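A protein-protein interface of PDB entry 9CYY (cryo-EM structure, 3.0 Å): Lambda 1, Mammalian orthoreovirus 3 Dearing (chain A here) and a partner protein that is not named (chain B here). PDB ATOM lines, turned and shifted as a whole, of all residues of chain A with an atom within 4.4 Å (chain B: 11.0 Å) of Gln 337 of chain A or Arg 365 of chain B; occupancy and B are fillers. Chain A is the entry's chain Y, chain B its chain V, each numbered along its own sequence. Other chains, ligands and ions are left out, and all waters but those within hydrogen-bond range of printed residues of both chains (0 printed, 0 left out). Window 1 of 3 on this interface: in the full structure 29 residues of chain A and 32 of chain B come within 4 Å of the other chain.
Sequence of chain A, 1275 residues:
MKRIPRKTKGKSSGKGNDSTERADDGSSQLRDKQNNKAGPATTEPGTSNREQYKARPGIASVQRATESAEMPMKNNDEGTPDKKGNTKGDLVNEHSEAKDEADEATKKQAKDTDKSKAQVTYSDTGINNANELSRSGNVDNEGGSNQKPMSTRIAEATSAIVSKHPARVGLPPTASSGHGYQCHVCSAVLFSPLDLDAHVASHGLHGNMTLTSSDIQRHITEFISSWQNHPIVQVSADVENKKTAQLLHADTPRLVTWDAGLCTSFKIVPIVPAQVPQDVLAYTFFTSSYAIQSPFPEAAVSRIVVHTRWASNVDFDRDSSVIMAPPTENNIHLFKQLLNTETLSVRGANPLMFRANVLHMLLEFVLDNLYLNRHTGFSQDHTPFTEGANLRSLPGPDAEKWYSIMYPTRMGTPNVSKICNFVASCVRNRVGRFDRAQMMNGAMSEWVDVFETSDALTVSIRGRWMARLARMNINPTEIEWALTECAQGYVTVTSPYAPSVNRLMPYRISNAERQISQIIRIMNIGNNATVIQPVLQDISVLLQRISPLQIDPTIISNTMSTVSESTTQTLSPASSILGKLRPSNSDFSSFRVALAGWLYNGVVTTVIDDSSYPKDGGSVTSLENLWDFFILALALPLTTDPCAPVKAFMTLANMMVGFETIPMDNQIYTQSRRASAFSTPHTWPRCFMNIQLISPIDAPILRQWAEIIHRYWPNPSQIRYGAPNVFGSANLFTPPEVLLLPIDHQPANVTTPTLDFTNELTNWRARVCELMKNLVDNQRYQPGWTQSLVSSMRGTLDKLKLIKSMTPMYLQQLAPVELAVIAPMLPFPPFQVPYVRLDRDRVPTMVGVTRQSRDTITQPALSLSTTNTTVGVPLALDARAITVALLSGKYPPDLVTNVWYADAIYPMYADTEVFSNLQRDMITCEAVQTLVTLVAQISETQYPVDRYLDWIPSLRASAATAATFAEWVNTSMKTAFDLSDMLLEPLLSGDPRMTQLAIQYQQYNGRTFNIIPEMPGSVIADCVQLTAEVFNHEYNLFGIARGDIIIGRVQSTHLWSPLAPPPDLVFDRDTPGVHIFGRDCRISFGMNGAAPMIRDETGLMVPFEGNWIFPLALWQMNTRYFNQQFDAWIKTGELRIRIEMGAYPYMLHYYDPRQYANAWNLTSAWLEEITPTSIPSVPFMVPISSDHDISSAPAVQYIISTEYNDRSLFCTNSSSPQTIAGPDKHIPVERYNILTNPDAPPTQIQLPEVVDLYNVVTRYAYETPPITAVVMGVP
The backbone NH of Gln 337 of chain A sits at hydrogen-bond distance from the side-chain amide oxygen of Asn 357 of chain A. The side-chain carboxylate (OD2) of Asp 363 of chain B lies within hydrogen-bond range of the backbone NH (N) of Arg 365 of chain B (3.3 Å). NE2 of Gln 337 of chain A is in hydrogen-bond range of O of His 333 of chain A (3.3 Å).
Among the printed residues, pairs that only touch across the chains: Ser 321 of chain A with Arg 365 of chain B and His 333 of chain A with Val 314 of chain B.
Printed residues of chain B within 4 Å of His 333 of chain A: Val 314. No residue of chain B comes within 4 Å of Lys 336 of chain A. Of chain B, only Arg 365 (3.2 Å) comes within 4 Å of Gln 337 of chain A. No residue of chain B comes within 4 Å of Leu 338 of chain A. No residue of chain B comes within 4 Å of Asn 340 of chain A. Printed residues of chain A within 4 Å of Val 314 of chain B: His 333 (3.4 Å). Arg 365 of chain B touches two residues of chain A. The nearest residue of chain B that does not touch Gln 337 of chain A is Thr 366 of chain B (5.8 Å).
Of the 21 printed residues of chain B, 2 touch a printed residue of chain A. Printed residues of chain B that touch a printed residue of chain A: Val 314 and Arg 365. Of the 11 printed residues of chain A, 3 touch a printed residue of chain B. Printed residues of chain A that touch a printed residue of chain B: Ser 321, His 333 and Gln 337. Hydrophobic or aromatic side chains of chain A within 4 Å of the printed part of chain B: His 333. Among the printed residues, 3 pairs touch across the chains.
NE of Arg 365 of chain B sits close to OE1 of Gln 337 of chain A (3.5 Å).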
ATOM      1  N   SER A 321      -4.711  22.694 -14.292  1.00  0.00           N
ATOM      2  CA  SER A 321      -5.169  21.365 -14.662  1.00  0.00           C
ATOM      3  C   SER A 321      -4.884  20.349 -13.559  1.00  0.00           C
ATOM      4  O   SER A 321      -3.945  20.488 -12.774  1.00  0.00           O
ATOM      5  CB  SER A 321      -4.506  20.923 -15.964  1.00  0.00           C
ATOM      6  OG  SER A 321      -3.133  20.644 -15.757  1.00  0.00           O
ATOM      7  N   HIS A 333       2.303  11.561  -5.944  1.00  0.00           N
ATOM      8  CA  HIS A 333       2.829  12.913  -6.092  1.00  0.00           C
ATOM      9  C   HIS A 333       1.728  13.960  -5.999  1.00  0.00           C
ATOM     10  O   HIS A 333       2.012  15.140  -5.764  1.00  0.00           O
ATOM     11  CB  HIS A 333       3.582  13.048  -7.414  1.00  0.00           C
ATOM     12  CG  HIS A 333       2.691  13.092  -8.615  1.00  0.00           C
ATOM     13  ND1 HIS A 333       2.158  14.265  -9.104  1.00  0.00           N
ATOM     14  CD2 HIS A 333       2.244  12.108  -9.431  1.00  0.00           C
ATOM     15  CE1 HIS A 333       1.419  14.002 -10.165  1.00  0.00           C
ATOM     16  NE2 HIS A 333       1.454  12.700 -10.385  1.00  0.00           N
ATOM     17  N   LEU A 334       0.471  13.555  -6.184  1.00  0.00           N
ATOM     18  CA  LEU A 334      -0.634  14.501  -6.103  1.00  0.00           C
ATOM     19  C   LEU A 334      -0.946  14.915  -4.672  1.00  0.00           C
ATOM     20  O   LEU A 334      -1.540  15.979  -4.467  1.00  0.00           O
ATOM     21  CB  LEU A 334      -1.881  13.905  -6.750  1.00  0.00           C
ATOM     22  CG  LEU A 334      -1.831  13.755  -8.269  1.00  0.00           C
ATOM     23  CD1 LEU A 334      -3.011  12.942  -8.757  1.00  0.00           C
ATOM     24  CD2 LEU A 334      -1.807  15.119  -8.933  1.00  0.00           C
ATOM     25  N   PHE A 335      -0.568  14.106  -3.683  1.00  0.00           N
ATOM     26  CA  PHE A 335      -0.895  14.371  -2.289  1.00  0.00           C
ATOM     27  C   PHE A 335       0.315  14.817  -1.478  1.00  0.00           C
ATOM     28  O   PHE A 335       0.288  14.746  -0.246  1.00  0.00           O
ATOM     29  CB  PHE A 335      -1.527  13.135  -1.650  1.00  0.00           C
ATOM     30  CG  PHE A 335      -2.567  12.479  -2.505  1.00  0.00           C
ATOM     31  CD1 PHE A 335      -3.773  13.107  -2.757  1.00  0.00           C
ATOM     32  CD2 PHE A 335      -2.339  11.231  -3.058  1.00  0.00           C
ATOM     33  CE1 PHE A 335      -4.731  12.503  -3.545  1.00  0.00           C
ATOM     34  CE2 PHE A 335      -3.294  10.623  -3.844  1.00  0.00           C
ATOM     35  CZ  PHE A 335      -4.491  11.260  -4.089  1.00  0.00           C
ATOM     36  N   LYS A 336       1.374  15.274  -2.137  1.00  0.00           N
ATOM     37  CA  LYS A 336       2.587  15.705  -1.456  1.00  0.00           C
ATOM     38  C   LYS A 336       3.087  17.026  -2.021  1.00  0.00           C
ATOM     39  O   LYS A 336       4.292  17.256  -2.155  1.00  0.00           O
ATOM     40  CB  LYS A 336       3.669  14.630  -1.536  1.00  0.00           C
ATOM     41  CG  LYS A 336       4.129  14.299  -2.941  1.00  0.00           C
ATOM     42  CD  LYS A 336       4.869  12.978  -2.976  1.00  0.00           C
ATOM     43  CE  LYS A 336       6.069  13.003  -2.051  1.00  0.00           C
ATOM     44  NZ  LYS A 336       7.115  13.949  -2.522  1.00  0.00           N
ATOM     45  N   GLN A 337       2.165  17.928  -2.338  1.00  0.00           N
ATOM     46  CA  GLN A 337       2.497  19.153  -3.046  1.00  0.00           C
ATOM     47  C   GLN A 337       2.745  20.345  -2.130  1.00  0.00           C
ATOM     48  O   GLN A 337       3.528  21.226  -2.493  1.00  0.00           O
ATOM     49  CB  GLN A 337       1.383  19.498  -4.037  1.00  0.00           C
ATOM     50  CG  GLN A 337       1.349  18.600  -5.255  1.00  0.00           C
ATOM     51  CD  GLN A 337       2.475  18.890  -6.220  1.00  0.00           C
ATOM     52  OE1 GLN A 337       2.448  19.886  -6.939  1.00  0.00           O
ATOM     53  NE2 GLN A 337       3.477  18.019  -6.240  1.00  0.00           N
ATOM     54  N   LEU A 338       2.114  20.398  -0.958  1.00  0.00           N
ATOM     55  CA  LEU A 338       2.105  21.645  -0.202  1.00  0.00           C
ATOM     56  C   LEU A 338       3.131  21.704   0.925  1.00  0.00           C
ATOM     57  O   LEU A 338       3.995  22.586   0.924  1.00  0.00           O
ATOM     58  CB  LEU A 338       0.708  21.902   0.367  1.00  0.00           C
ATOM     59  CG  LEU A 338      -0.251  22.688  -0.526  1.00  0.00           C
ATOM     60  CD1 LEU A 338      -0.742  21.843  -1.687  1.00  0.00           C
ATOM     61  CD2 LEU A 338      -1.419  23.217   0.287  1.00  0.00           C
ATOM     62  N   LEU A 339       3.059  20.785   1.887  1.00  0.00           N
ATOM     63  CA  LEU A 339       3.877  20.885   3.091  1.00  0.00           C
ATOM     64  C   LEU A 339       4.771  19.671   3.307  1.00  0.00           C
ATOM     65  O   LEU A 339       5.233  19.440   4.427  1.00  0.00           O
ATOM     66  CB  LEU A 339       2.993  21.109   4.319  1.00  0.00           C
ATOM     67  CG  LEU A 339       2.568  22.547   4.625  1.00  0.00           C
ATOM     68  CD1 LEU A 339       1.425  22.989   3.731  1.00  0.00           C
ATOM     69  CD2 LEU A 339       2.185  22.690   6.084  1.00  0.00           C
ATOM     70  N   ASN A 340       5.028  18.890   2.261  1.00  0.00           N
ATOM     71  CA  ASN A 340       5.913  17.732   2.370  1.00  0.00           C
ATOM     72  C   ASN A 340       7.323  18.109   1.915  1.00  0.00           C
ATOM     73  O   ASN A 340       7.903  17.529   0.998  1.00  0.00           O
ATOM     74  CB  ASN A 340       5.349  16.561   1.578  1.00  0.00           C
ATOM     75  CG  ASN A 340       4.041  16.072   2.145  1.00  0.00           C
ATOM     76  OD1 ASN A 340       2.994  16.184   1.519  1.00  0.00           O
ATOM     77  ND2 ASN A 340       4.097  15.525   3.345  1.00  0.00           N
ATOM     78  N   ASN A 357      -3.865  19.071   1.090  1.00  0.00           N
ATOM     79  CA  ASN A 357      -3.613  18.739  -0.308  1.00  0.00           C
ATOM     80  C   ASN A 357      -4.916  18.555  -1.076  1.00  0.00           C
ATOM     81  O   ASN A 357      -5.043  19.016  -2.217  1.00  0.00           O
ATOM     82  CB  ASN A 357      -2.748  17.485  -0.397  1.00  0.00           C
ATOM     83  CG  ASN A 357      -1.296  17.763  -0.072  1.00  0.00           C
ATOM     84  OD1 ASN A 357      -0.478  17.973  -0.966  1.00  0.00           O
ATOM     85  ND2 ASN A 357      -0.969  17.770   1.212  1.00  0.00           N
ATOM     86  N   TRP A 968      -0.274  29.676  -0.832  1.00  0.00           N
ATOM     87  CA  TRP A 968      -0.556  28.765  -1.937  1.00  0.00           C
ATOM     88  C   TRP A 968      -1.856  29.131  -2.642  1.00  0.00           C
ATOM     89  O   TRP A 968      -1.924  29.121  -3.877  1.00  0.00           O
ATOM     90  CB  TRP A 968      -0.604  27.323  -1.437  1.00  0.00           C
ATOM     91  CG  TRP A 968       0.732  26.661  -1.418  1.00  0.00           C
ATOM     92  CD1 TRP A 968       1.650  26.696  -0.413  1.00  0.00           C
ATOM     93  CD2 TRP A 968       1.308  25.871  -2.461  1.00  0.00           C
ATOM     94  NE1 TRP A 968       2.761  25.970  -0.762  1.00  0.00           N
ATOM     95  CE2 TRP A 968       2.576  25.453  -2.017  1.00  0.00           C
ATOM     96  CE3 TRP A 968       0.873  25.471  -3.728  1.00  0.00           C
ATOM     97  CZ2 TRP A 968       3.413  24.658  -2.792  1.00  0.00           C
ATOM     98  CZ3 TRP A 968       1.704  24.682  -4.495  1.00  0.00           C
ATOM     99  CH2 TRP A 968       2.961  24.284  -4.026  1.00  0.00           C
ATOM    100  N   LEU B 301       8.918  20.338 -23.149  1.00  0.00           N
ATOM    101  CA  LEU B 301       8.228  19.917 -21.939  1.00  0.00           C
ATOM    102  C   LEU B 301       8.538  18.450 -21.690  1.00  0.00           C
ATOM    103  O   LEU B 301       8.407  17.623 -22.600  1.00  0.00           O
ATOM    104  CB  LEU B 301       6.717  20.116 -22.074  1.00  0.00           C
ATOM    105  CG  LEU B 301       6.206  21.535 -22.320  1.00  0.00           C
ATOM    106  CD1 LEU B 301       4.714  21.511 -22.598  1.00  0.00           C
ATOM    107  CD2 LEU B 301       6.515  22.438 -21.145  1.00  0.00           C
ATOM    108  N   PHE B 302       8.943  18.118 -20.466  1.00  0.00           N
ATOM    109  CA  PHE B 302       9.189  16.719 -20.159  1.00  0.00           C
ATOM    110  C   PHE B 302       8.876  16.456 -18.695  1.00  0.00           C
ATOM    111  O   PHE B 302       8.614  17.374 -17.913  1.00  0.00           O
ATOM    112  CB  PHE B 302      10.626  16.299 -20.504  1.00  0.00           C
ATOM    113  CG  PHE B 302      11.684  16.993 -19.697  1.00  0.00           C
ATOM    114  CD1 PHE B 302      12.106  18.267 -20.032  1.00  0.00           C
ATOM    115  CD2 PHE B 302      12.279  16.356 -18.622  1.00  0.00           C
ATOM    116  CE1 PHE B 302      13.086  18.903 -19.296  1.00  0.00           C
ATOM    117  CE2 PHE B 302      13.261  16.985 -17.884  1.00  0.00           C
ATOM    118  CZ  PHE B 302      13.665  18.260 -18.222  1.00  0.00           C
ATOM    119  N   GLU B 303       8.870  15.173 -18.347  1.00  0.00           N
ATOM    120  CA  GLU B 303       8.530  14.733 -17.003  1.00  0.00           C
ATOM    121  C   GLU B 303       9.508  13.659 -16.556  1.00  0.00           C
ATOM    122  O   GLU B 303       9.895  12.793 -17.347  1.00  0.00           O
ATOM    123  CB  GLU B 303       7.086  14.218 -16.948  1.00  0.00           C
ATOM    124  CG  GLU B 303       6.830  12.965 -17.765  1.00  0.00           C
ATOM    125  CD  GLU B 303       5.378  12.533 -17.734  1.00  0.00           C
ATOM    126  OE1 GLU B 303       4.564  13.227 -17.091  1.00  0.00           O
ATOM    127  OE2 GLU B 303       5.050  11.501 -18.356  1.00  0.00           O
ATOM    128  N   ASN B 313       6.117   5.917 -11.969  1.00  0.00           N
ATOM    129  CA  ASN B 313       5.849   6.918 -10.934  1.00  0.00           C
ATOM    130  C   ASN B 313       6.349   8.265 -11.468  1.00  0.00           C
ATOM    131  O   ASN B 313       7.552   8.472 -11.617  1.00  0.00           O
ATOM    132  CB  ASN B 313       6.516   6.553  -9.621  1.00  0.00           C
ATOM    133  CG  ASN B 313       6.188   7.526  -8.503  1.00  0.00           C
ATOM    134  OD1 ASN B 313       5.480   8.511  -8.702  1.00  0.00           O
ATOM    135  ND2 ASN B 313       6.707   7.248  -7.314  1.00  0.00           N
ATOM    136  N   VAL B 314       5.409   9.163 -11.758  1.00  0.00           N
ATOM    137  CA  VAL B 314       5.755  10.497 -12.237  1.00  0.00           C
ATOM    138  C   VAL B 314       6.215  11.337 -11.056  1.00  0.00           C
ATOM    139  O   VAL B 314       5.477  11.511 -10.080  1.00  0.00           O
ATOM    140  CB  VAL B 314       4.568  11.158 -12.960  1.00  0.00           C
ATOM    141  CG1 VAL B 314       5.006  12.459 -13.608  1.00  0.00           C
ATOM    142  CG2 VAL B 314       3.986  10.210 -13.993  1.00  0.00           C
ATOM    143  N   SER B 315       7.440  11.863 -11.129  1.00  0.00           N
ATOM    144  CA  SER B 315       8.001  12.576  -9.988  1.00  0.00           C
ATOM    145  C   SER B 315       7.862  14.086 -10.142  1.00  0.00           C
ATOM    146  O   SER B 315       7.468  14.774  -9.194  1.00  0.00           O
ATOM    147  CB  SER B 315       9.467  12.191  -9.802  1.00  0.00           C
ATOM    148  OG  SER B 315      10.045  12.899  -8.719  1.00  0.00           O
ATOM    149  N   ARG B 316       8.181  14.623 -11.318  1.00  0.00           N
ATOM    150  CA  ARG B 316       8.255  16.069 -11.466  1.00  0.00           C
ATOM    151  C   ARG B 316       8.025  16.453 -12.921  1.00  0.00           C
ATOM    152  O   ARG B 316       8.282  15.669 -13.839  1.00  0.00           O
ATOM    153  CB  ARG B 316       9.604  16.599 -10.971  1.00  0.00           C
ATOM    154  CG  ARG B 316       9.589  18.054 -10.560  1.00  0.00           C
ATOM    155  CD  ARG B 316      10.995  18.565 -10.306  1.00  0.00           C
ATOM    156  NE  ARG B 316      11.635  17.868  -9.197  1.00  0.00           N
ATOM    157  CZ  ARG B 316      11.578  18.265  -7.932  1.00  0.00           C
ATOM    158  NH1 ARG B 316      10.915  19.353  -7.578  1.00  0.00           N
ATOM    159  NH2 ARG B 316      12.202  17.549  -7.000  1.00  0.00           N
ATOM    160  N   LYS B 317       7.547  17.683 -13.112  1.00  0.00           N
ATOM    161  CA  LYS B 317       7.239  18.239 -14.423  1.00  0.00           C
ATOM    162  C   LYS B 317       8.172  19.411 -14.696  1.00  0.00           C
ATOM    163  O   LYS B 317       8.160  20.400 -13.955  1.00  0.00           O
ATOM    164  CB  LYS B 317       5.786  18.717 -14.486  1.00  0.00           C
ATOM    165  CG  LYS B 317       4.741  17.638 -14.268  1.00  0.00           C
ATOM    166  CD  LYS B 317       4.692  16.647 -15.409  1.00  0.00           C
ATOM    167  CE  LYS B 317       3.639  15.586 -15.147  1.00  0.00           C
ATOM    168  NZ  LYS B 317       2.264  16.155 -15.190  1.00  0.00           N
ATOM    169  N   LEU B 318       8.952  19.321 -15.772  1.00  0.00           N
ATOM    170  CA  LEU B 318       9.968  20.319 -16.061  1.00  0.00           C
ATOM    171  C   LEU B 318       9.788  20.863 -17.470  1.00  0.00           C
ATOM    172  O   LEU B 318       9.304  20.174 -18.376  1.00  0.00           O
ATOM    173  CB  LEU B 318      11.377  19.733 -15.900  1.00  0.00           C
ATOM    174  CG  LEU B 318      11.720  19.210 -14.506  1.00  0.00           C
ATOM    175  CD1 LEU B 318      13.027  18.438 -14.529  1.00  0.00           C
ATOM    176  CD2 LEU B 318      11.788  20.355 -13.510  1.00  0.00           C
ATOM    177  N   THR B 319      10.178  22.125 -17.641  1.00  0.00           N
ATOM    178  CA  THR B 319      10.217  22.759 -18.951  1.00  0.00           C
ATOM    179  C   THR B 319      11.603  23.345 -19.172  1.00  0.00           C
ATOM    180  O   THR B 319      12.115  24.082 -18.325  1.00  0.00           O
ATOM    181  CB  THR B 319       9.132  23.839 -19.086  1.00  0.00           C
ATOM    182  OG1 THR B 319       9.254  24.492 -20.356  1.00  0.00           O
ATOM    183  CG2 THR B 319       9.215  24.868 -17.963  1.00  0.00           C
ATOM    184  N   HIS B 321      14.115  25.620 -21.593  1.00  0.00           N
ATOM    185  CA  HIS B 321      13.835  26.799 -22.399  1.00  0.00           C
ATOM    186  C   HIS B 321      14.867  27.008 -23.498  1.00  0.00           C
ATOM    187  O   HIS B 321      16.046  26.675 -23.344  1.00  0.00           O
ATOM    188  CB  HIS B 321      13.775  28.057 -21.526  1.00  0.00           C
ATOM    189  CG  HIS B 321      12.873  27.923 -20.339  1.00  0.00           C
ATOM    190  ND1 HIS B 321      11.606  28.464 -20.304  1.00  0.00           N
ATOM    191  CD2 HIS B 321      13.052  27.307 -19.148  1.00  0.00           C
ATOM    192  CE1 HIS B 321      11.044  28.189 -19.141  1.00  0.00           C
ATOM    193  NE2 HIS B 321      11.901  27.487 -18.421  1.00  0.00           N
ATOM    194  N   LEU B 361      16.133  25.228 -16.911  1.00  0.00           N
ATOM    195  CA  LEU B 361      14.988  24.374 -16.632  1.00  0.00           C
ATOM    196  C   LEU B 361      14.155  25.013 -15.532  1.00  0.00           C
ATOM    197  O   LEU B 361      14.703  25.507 -14.542  1.00  0.00           O
ATOM    198  CB  LEU B 361      15.423  22.968 -16.194  1.00  0.00           C
ATOM    199  CG  LEU B 361      15.917  21.940 -17.215  1.00  0.00           C
ATOM    200  CD1 LEU B 361      17.206  22.380 -17.889  1.00  0.00           C
ATOM    201  CD2 LEU B 361      16.095  20.586 -16.553  1.00  0.00           C
ATOM    202  N   THR B 362      12.838  24.982 -15.695  1.00  0.00           N
ATOM    203  CA  THR B 362      11.908  25.521 -14.715  1.00  0.00           C
ATOM    204  C   THR B 362      10.909  24.446 -14.312  1.00  0.00           C
ATOM    205  O   THR B 362      10.428  23.680 -15.158  1.00  0.00           O
ATOM    206  CB  THR B 362      11.167  26.742 -15.269  1.00  0.00           C
ATOM    207  OG1 THR B 362      12.111  27.658 -15.837  1.00  0.00           O
ATOM    208  CG2 THR B 362      10.397  27.448 -14.164  1.00  0.00           C
ATOM    209  N   ASP B 363      10.610  24.383 -13.016  1.00  0.00           N
ATOM    210  CA  ASP B 363       9.568  23.492 -12.523  1.00  0.00           C
ATOM    211  C   ASP B 363       8.202  24.041 -12.911  1.00  0.00           C
ATOM    212  O   ASP B 363       7.928  25.230 -12.723  1.00  0.00           O
ATOM    213  CB  ASP B 363       9.670  23.338 -11.006  1.00  0.00           C
ATOM    214  CG  ASP B 363       8.696  22.317 -10.460  1.00  0.00           C
ATOM    215  OD1 ASP B 363       8.937  21.109 -10.647  1.00  0.00           O
ATOM    216  OD2 ASP B 363       7.688  22.723  -9.846  1.00  0.00           O
ATOM    217  N   ARG B 364       7.340  23.177 -13.453  1.00  0.00           N
ATOM    218  CA  ARG B 364       6.073  23.662 -13.992  1.00  0.00           C
ATOM    219  C   ARG B 364       5.084  24.001 -12.882  1.00  0.00           C
ATOM    220  O   ARG B 364       4.316  24.962 -12.999  1.00  0.00           O
ATOM    221  CB  ARG B 364       5.485  22.635 -14.960  1.00  0.00           C
ATOM    222  CG  ARG B 364       6.177  22.634 -16.314  1.00  0.00           C
ATOM    223  CD  ARG B 364       5.263  22.150 -17.427  1.00  0.00           C
ATOM    224  NE  ARG B 364       5.036  20.712 -17.382  1.00  0.00           N
ATOM    225  CZ  ARG B 364       5.781  19.818 -18.018  1.00  0.00           C
ATOM    226  NH1 ARG B 364       6.837  20.180 -18.728  1.00  0.00           N
ATOM    227  NH2 ARG B 364       5.459  18.532 -17.940  1.00  0.00           N
ATOM    228  N   ARG B 365       5.081  23.226 -11.796  1.00  0.00           N
ATOM    229  CA  ARG B 365       4.156  23.505 -10.702  1.00  0.00           C
ATOM    230  C   ARG B 365       4.597  24.730  -9.910  1.00  0.00           C
ATOM    231  O   ARG B 365       3.887  25.741  -9.855  1.00  0.00           O
ATOM    232  CB  ARG B 365       4.035  22.285  -9.789  1.00  0.00           C
ATOM    233  CG  ARG B 365       3.109  22.510  -8.605  1.00  0.00           C
ATOM    234  CD  ARG B 365       1.672  22.715  -9.057  1.00  0.00           C
ATOM    235  NE  ARG B 365       1.111  21.525  -9.684  1.00  0.00           N
ATOM    236  CZ  ARG B 365      -0.024  21.505 -10.368  1.00  0.00           C
ATOM    237  NH1 ARG B 365      -0.748  22.598 -10.540  1.00  0.00           N
ATOM    238  NH2 ARG B 365      -0.444  20.357 -10.895  1.00  0.00           N
ATOM    239  N   THR B 366       5.770  24.658  -9.288  1.00  0.00           N
ATOM    240  CA  THR B 366       6.365  25.797  -8.601  1.00  0.00           C
ATOM    241  C   THR B 366       7.288  26.495  -9.592  1.00  0.00           C
ATOM    242  O   THR B 366       8.325  25.946  -9.973  1.00  0.00           O
ATOM    243  CB  THR B 366       7.129  25.358  -7.353  1.00  0.00           C
ATOM    244  OG1 THR B 366       8.275  24.591  -7.738  1.00  0.00           O
ATOM    245  CG2 THR B 366       6.239  24.510  -6.462  1.00  0.00           C
ATOM    246  N   HIS B 367       6.920  27.707  -9.995  1.00  0.00           N
ATOM    247  CA  HIS B 367       7.633  28.382 -11.071  1.00  0.00           C
ATOM    248  C   HIS B 367       9.005  28.843 -10.599  1.00  0.00           C
ATOM    249  O   HIS B 367       9.232  30.038 -10.387  1.00  0.00           O
ATOM    250  CB  HIS B 367       6.809  29.560 -11.590  1.00  0.00           C
ATOM    251  CG  HIS B 367       5.366  29.228 -11.808  1.00  0.00           C
ATOM    252  ND1 HIS B 367       4.943  28.369 -12.800  1.00  0.00           N
ATOM    253  CD2 HIS B 367       4.249  29.629 -11.156  1.00  0.00           C
ATOM    254  CE1 HIS B 367       3.627  28.261 -12.754  1.00  0.00           C
ATOM    255  NE2 HIS B 367       3.182  29.015 -11.764  1.00  0.00           N
ATOM    256  N   CYS B 368       9.924  27.894 -10.438  1.00  0.00           N
ATOM    257  CA  CYS B 368      11.261  28.168  -9.938  1.00  0.00           C
ATOM    258  C   CYS B 368      12.295  27.452 -10.795  1.00  0.00           C
ATOM    259  O   CYS B 368      12.014  26.416 -11.411  1.00  0.00           O
ATOM    260  CB  CYS B 368      11.409  27.736  -8.473  1.00  0.00           C
ATOM    261  SG  CYS B 368      13.031  28.075  -7.752  1.00  0.00           S
ATOM    262  N   GLN B 369      13.498  28.021 -10.821  1.00  0.00           N
ATOM    263  CA  GLN B 369      14.609  27.411 -11.535  1.00  0.00           C
ATOM    264  C   GLN B 369      14.980  26.081 -10.893  1.00  0.00           C
ATOM    265  O   GLN B 369      15.010  25.952  -9.666  1.00  0.00           O
ATOM    266  CB  GLN B 369      15.815  28.351 -11.534  1.00  0.00           C
ATOM    267  CG  GLN B 369      15.795  29.404 -12.630  1.00  0.00           C
ATOM    268  CD  GLN B 369      15.711  28.806 -14.020  1.00  0.00           C
ATOM    269  OE1 GLN B 369      16.327  27.779 -14.305  1.00  0.00           O
ATOM    270  NE2 GLN B 369      14.946  29.447 -14.895  1.00  0.00           N
ATOM    271  N   TYR B 370      15.265  25.087 -11.728  1.00  0.00           N
ATOM    272  CA  TYR B 370      15.598  23.746 -11.270  1.00  0.00           C
ATOM    273  C   TYR B 370      17.049  23.439 -11.610  1.00  0.00           C
ATOM    274  O   TYR B 370      17.495  23.696 -12.732  1.00  0.00           O
ATOM    275  CB  TYR B 370      14.674  22.707 -11.907  1.00  0.00           C
ATOM    276  CG  TYR B 370      14.928  21.297 -11.432  1.00  0.00           C
ATOM    277  CD1 TYR B 370      14.809  20.965 -10.090  1.00  0.00           C
ATOM    278  CD2 TYR B 370      15.282  20.298 -12.326  1.00  0.00           C
ATOM    279  CE1 TYR B 370      15.039  19.677  -9.651  1.00  0.00           C
ATOM    280  CE2 TYR B 370      15.514  19.007 -11.897  1.00  0.00           C
ATOM    281  CZ  TYR B 370      15.391  18.702 -10.559  1.00  0.00           C
ATOM    282  OH  TYR B 370      15.621  17.417 -10.126  1.00  0.00           O
